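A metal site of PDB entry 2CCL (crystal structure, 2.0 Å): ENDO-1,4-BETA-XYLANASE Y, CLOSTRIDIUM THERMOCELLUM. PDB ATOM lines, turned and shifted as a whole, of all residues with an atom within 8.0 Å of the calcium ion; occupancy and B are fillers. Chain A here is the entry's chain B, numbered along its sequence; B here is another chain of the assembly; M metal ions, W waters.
OD2 of Asp 17 sits close to N of Asn 14, 3.0 Å away.
The side-chain carboxylate (OD1) of Asp 17 sits close to the backbone NH (N) of Val 7.
NE of Arg 38 sits at hydrogen-bond distance from O of Asp 6 (2.8 Å).
OD2 of Asp 6 lies within hydrogen-bond range of N of Gly 11, at 2.8 Å.
N of Gly 9 lies close to OD1 of Asp 6 (3.3 Å).
The calcium ion is bound by the side-chain carboxylate (OD1) of Asp 6 (2.3 Å), the backbone carbonyl oxygen (O) of Thr 12 (2.3 Å), the side-chain carboxylate (OD1) of Asp 10 (2.4 Å), the side-chain carboxylate (OD2) of Asp 17 (2.4 Å), the side-chain amide oxygen (OD1) of Asn 8 (2.5 Å), water W1 (2.5 Å) and the side-chain carboxylate (OD1) of Asp 17 (2.5 Å).
The calcium ion has seven donor atoms within binding distance.
Water W1 lies within hydrogen-bond range of OD1 of Asn 14 (2.7 Å), OD2 of Asp 10 (2.9 Å) and ND2 of Asn 8 (3.2 Å).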
ATOM      1  N   LEU A   3     -21.298  -7.212 -18.251  1.00  0.00           N
ATOM      2  CA  LEU A   3     -20.246  -7.261 -19.272  1.00  0.00           C
ATOM      3  C   LEU A   3     -18.854  -7.120 -18.647  1.00  0.00           C
ATOM      4  O   LEU A   3     -18.345  -6.008 -18.458  1.00  0.00           O
ATOM      5  CB  LEU A   3     -20.476  -6.213 -20.376  1.00  0.00           C
ATOM      6  CG  LEU A   3     -19.579  -6.290 -21.624  1.00  0.00           C
ATOM      7  CD1 LEU A   3     -19.809  -7.592 -22.403  1.00  0.00           C
ATOM      8  CD2 LEU A   3     -19.775  -5.082 -22.518  1.00  0.00           C
ATOM      9  N   GLY A   5     -15.092  -6.788 -17.867  1.00  0.00           N
ATOM     10  CA  GLY A   5     -14.035  -6.033 -18.547  1.00  0.00           C
ATOM     11  C   GLY A   5     -14.440  -4.634 -18.952  1.00  0.00           C
ATOM     12  O   GLY A   5     -13.589  -3.777 -19.152  1.00  0.00           O
ATOM     13  N   ASP A   6     -15.748  -4.396 -19.097  1.00  0.00           N
ATOM     14  CA  ASP A   6     -16.265  -3.091 -19.472  1.00  0.00           C
ATOM     15  C   ASP A   6     -16.378  -2.180 -18.246  1.00  0.00           C
ATOM     16  O   ASP A   6     -17.481  -1.761 -17.866  1.00  0.00           O
ATOM     17  CB  ASP A   6     -17.616  -3.230 -20.198  1.00  0.00           C
ATOM     18  CG  ASP A   6     -18.185  -1.894 -20.646  1.00  0.00           C
ATOM     19  OD1 ASP A   6     -17.417  -0.923 -20.813  1.00  0.00           O
ATOM     20  OD2 ASP A   6     -19.411  -1.815 -20.852  1.00  0.00           O
ATOM     21  N   VAL A   7     -15.233  -1.845 -17.656  1.00  0.00           N
ATOM     22  CA  VAL A   7     -15.183  -1.107 -16.402  1.00  0.00           C
ATOM     23  C   VAL A   7     -16.094   0.143 -16.394  1.00  0.00           C
ATOM     24  O   VAL A   7     -16.908   0.285 -15.493  1.00  0.00           O
ATOM     25  CB  VAL A   7     -13.721  -0.722 -16.030  1.00  0.00           C
ATOM     26  CG1 VAL A   7     -13.691  -0.036 -14.663  1.00  0.00           C
ATOM     27  CG2 VAL A   7     -12.822  -1.955 -16.016  1.00  0.00           C
ATOM     28  N   ASN A   8     -15.971   0.998 -17.404  1.00  0.00           N
ATOM     29  CA  ASN A   8     -16.737   2.253 -17.438  1.00  0.00           C
ATOM     30  C   ASN A   8     -18.193   2.105 -17.903  1.00  0.00           C
ATOM     31  O   ASN A   8     -18.954   3.075 -17.899  1.00  0.00           O
ATOM     32  CB  ASN A   8     -16.004   3.342 -18.239  1.00  0.00           C
ATOM     33  CG  ASN A   8     -15.954   3.062 -19.734  1.00  0.00           C
ATOM     34  OD1 ASN A   8     -16.531   2.086 -20.212  1.00  0.00           O
ATOM     35  ND2 ASN A   8     -15.268   3.917 -20.472  1.00  0.00           N
ATOM     36  N   GLY A   9     -18.553   0.897 -18.327  1.00  0.00           N
ATOM     37  CA  GLY A   9     -19.927   0.574 -18.717  1.00  0.00           C
ATOM     38  C   GLY A   9     -20.451   1.213 -19.986  1.00  0.00           C
ATOM     39  O   GLY A   9     -21.655   1.407 -20.121  1.00  0.00           O
ATOM     40  N   ASP A  10     -19.565   1.540 -20.922  1.00  0.00           N
ATOM     41  CA  ASP A  10     -19.996   2.140 -22.191  1.00  0.00           C
ATOM     42  C   ASP A  10     -20.324   1.119 -23.284  1.00  0.00           C
ATOM     43  O   ASP A  10     -20.582   1.492 -24.435  1.00  0.00           O
ATOM     44  CB  ASP A  10     -18.991   3.191 -22.705  1.00  0.00           C
ATOM     45  CG  ASP A  10     -17.663   2.595 -23.118  1.00  0.00           C
ATOM     46  OD1 ASP A  10     -17.481   1.370 -23.007  1.00  0.00           O
ATOM     47  OD2 ASP A  10     -16.784   3.370 -23.541  1.00  0.00           O
ATOM     48  N   GLY A  11     -20.305  -0.166 -22.924  1.00  0.00           N
ATOM     49  CA  GLY A  11     -20.751  -1.237 -23.815  1.00  0.00           C
ATOM     50  C   GLY A  11     -19.671  -1.862 -24.670  1.00  0.00           C
ATOM     51  O   GLY A  11     -19.940  -2.799 -25.427  1.00  0.00           O
ATOM     52  N   THR A  12     -18.453  -1.346 -24.566  1.00  0.00           N
ATOM     53  CA  THR A  12     -17.308  -1.919 -25.284  1.00  0.00           C
ATOM     54  C   THR A  12     -16.115  -2.051 -24.349  1.00  0.00           C
ATOM     55  O   THR A  12     -15.924  -1.239 -23.435  1.00  0.00           O
ATOM     56  CB  THR A  12     -16.944  -1.096 -26.560  1.00  0.00           C
ATOM     57  OG1 THR A  12     -15.874  -1.745 -27.260  1.00  0.00           O
ATOM     58  CG2 THR A  12     -16.516   0.326 -26.211  1.00  0.00           C
ATOM     59  N   ILE A  13     -15.326  -3.101 -24.554  1.00  0.00           N
ATOM     60  CA  ILE A  13     -14.123  -3.351 -23.749  1.00  0.00           C
ATOM     61  C   ILE A  13     -12.878  -2.874 -24.496  1.00  0.00           C
ATOM     62  O   ILE A  13     -12.551  -3.393 -25.562  1.00  0.00           O
ATOM     63  CB  ILE A  13     -13.971  -4.853 -23.388  1.00  0.00           C
ATOM     64  CG1 ILE A  13     -15.265  -5.392 -22.746  1.00  0.00           C
ATOM     65  CG2 ILE A  13     -12.767  -5.070 -22.468  1.00  0.00           C
ATOM     66  CD1 ILE A  13     -15.395  -6.898 -22.824  1.00  0.00           C
ATOM     67  N   ASN A  14     -12.208  -1.880 -23.938  1.00  0.00           N
ATOM     68  CA  ASN A  14     -10.986  -1.321 -24.534  1.00  0.00           C
ATOM     69  C   ASN A  14      -9.986  -0.795 -23.506  1.00  0.00           C
ATOM     70  O   ASN A  14     -10.211  -0.919 -22.288  1.00  0.00           O
ATOM     71  CB  ASN A  14     -11.311  -0.261 -25.613  1.00  0.00           C
ATOM     72  CG  ASN A  14     -12.102   0.924 -25.078  1.00  0.00           C
ATOM     73  OD1 ASN A  14     -11.921   1.358 -23.937  1.00  0.00           O
ATOM     74  ND2 ASN A  14     -12.987   1.474 -25.917  1.00  0.00           N
ATOM     75  N   SER A  15      -8.886  -0.216 -23.987  1.00  0.00           N
ATOM     76  CA  SER A  15      -7.800   0.255 -23.138  1.00  0.00           C
ATOM     77  C   SER A  15      -8.178   1.386 -22.173  1.00  0.00           C
ATOM     78  O   SER A  15      -7.453   1.657 -21.221  1.00  0.00           O
ATOM     79  CB  SER A  15      -6.580   0.653 -23.980  1.00  0.00           C
ATOM     80  OG  SER A  15      -6.903   1.627 -24.953  1.00  0.00           O
ATOM     81  N   THR A  16      -9.317   2.041 -22.419  1.00  0.00           N
ATOM     82  CA  THR A  16      -9.799   3.105 -21.521  1.00  0.00           C
ATOM     83  C   THR A  16     -10.318   2.493 -20.222  1.00  0.00           C
ATOM     84  O   THR A  16     -10.123   3.054 -19.142  1.00  0.00           O
ATOM     85  CB  THR A  16     -10.852   3.994 -22.222  1.00  0.00           C
ATOM     86  OG1 THR A  16     -10.332   4.437 -23.484  1.00  0.00           O
ATOM     87  CG2 THR A  16     -11.201   5.222 -21.370  1.00  0.00           C
ATOM     88  N   ASP A  17     -10.956   1.326 -20.343  1.00  0.00           N
ATOM     89  CA  ASP A  17     -11.314   0.515 -19.181  1.00  0.00           C
ATOM     90  C   ASP A  17     -10.075   0.082 -18.405  1.00  0.00           C
ATOM     91  O   ASP A  17     -10.084   0.067 -17.164  1.00  0.00           O
ATOM     92  CB  ASP A  17     -12.100  -0.717 -19.597  1.00  0.00           C
ATOM     93  CG  ASP A  17     -13.395  -0.381 -20.294  1.00  0.00           C
ATOM     94  OD1 ASP A  17     -14.237   0.315 -19.679  1.00  0.00           O
ATOM     95  OD2 ASP A  17     -13.566  -0.794 -21.460  1.00  0.00           O
ATOM     96  N   LEU A  18      -9.020  -0.278 -19.130  1.00  0.00           N
ATOM     97  CA  LEU A  18      -7.742  -0.646 -18.505  1.00  0.00           C
ATOM     98  C   LEU A  18      -7.146   0.498 -17.675  1.00  0.00           C
ATOM     99  O   LEU A  18      -6.742   0.279 -16.525  1.00  0.00           O
ATOM    100  CB  LEU A  18      -6.733  -1.157 -19.543  1.00  0.00           C
ATOM    101  CG  LEU A  18      -5.403  -1.723 -19.019  1.00  0.00           C
ATOM    102  CD1 LEU A  18      -5.615  -2.854 -18.005  1.00  0.00           C
ATOM    103  CD2 LEU A  18      -4.537  -2.178 -20.160  1.00  0.00           C
ATOM    104  N   MET A  20      -8.793   3.013 -16.383  1.00  0.00           N
ATOM    105  CA  MET A  20      -9.709   3.145 -15.256  1.00  0.00           C
ATOM    106  C   MET A  20      -9.458   2.087 -14.193  1.00  0.00           C
ATOM    107  O   MET A  20      -9.425   2.396 -13.004  1.00  0.00           O
ATOM    108  CB  MET A  20     -11.158   3.083 -15.738  1.00  0.00           C
ATOM    109  CG  MET A  20     -12.103   3.852 -14.851  1.00  0.00           C
ATOM    110  SD  MET A  20     -13.814   3.746 -15.365  1.00  0.00           S
ATOM    111  CE  MET A  20     -14.446   5.264 -14.668  1.00  0.00           C
ATOM    112  N   ARG A  38     -18.039  -5.126 -13.003  1.00  0.00           N
ATOM    113  CA  ARG A  38     -17.456  -5.242 -14.343  1.00  0.00           C
ATOM    114  C   ARG A  38     -15.921  -5.341 -14.286  1.00  0.00           C
ATOM    115  O   ARG A  38     -15.310  -5.960 -15.152  1.00  0.00           O
ATOM    116  CB  ARG A  38     -17.913  -4.088 -15.242  1.00  0.00           C
ATOM    117  CG  ARG A  38     -19.437  -3.940 -15.313  1.00  0.00           C
ATOM    118  CD  ARG A  38     -19.891  -2.910 -16.336  1.00  0.00           C
ATOM    119  NE  ARG A  38     -19.477  -1.553 -15.976  1.00  0.00           N
ATOM    120  CZ  ARG A  38     -20.263  -0.651 -15.403  1.00  0.00           C
ATOM    121  NH1 ARG A  38     -21.530  -0.936 -15.117  1.00  0.00           N
ATOM    122  NH2 ARG A  38     -19.772   0.557 -15.118  1.00  0.00           N
ATOM    123  N   GLU B 131     -12.248  10.018 -24.631  1.00  0.00           N
ATOM    124  CA  GLU B 131     -11.937   9.302 -25.864  1.00  0.00           C
ATOM    125  C   GLU B 131     -11.753  10.267 -27.029  1.00  0.00           C
ATOM    126  O   GLU B 131     -12.506  11.224 -27.163  1.00  0.00           O
ATOM    127  CB  GLU B 131     -13.047   8.298 -26.203  1.00  0.00           C
ATOM    128  CG  GLU B 131     -13.123   7.095 -25.263  1.00  0.00           C
ATOM    129  CD  GLU B 131     -12.175   5.975 -25.647  1.00  0.00           C
ATOM    130  OE1 GLU B 131     -11.324   6.183 -26.540  1.00  0.00           O
ATOM    131  OE2 GLU B 131     -12.284   4.882 -25.057  1.00  0.00           O
HETATM  132 CA    CA M   1     -15.718   0.319 -21.747  1.00  0.00          CA
HETATM  133  O   HOH W   1     -14.331   2.034 -22.891  1.00  0.00           O
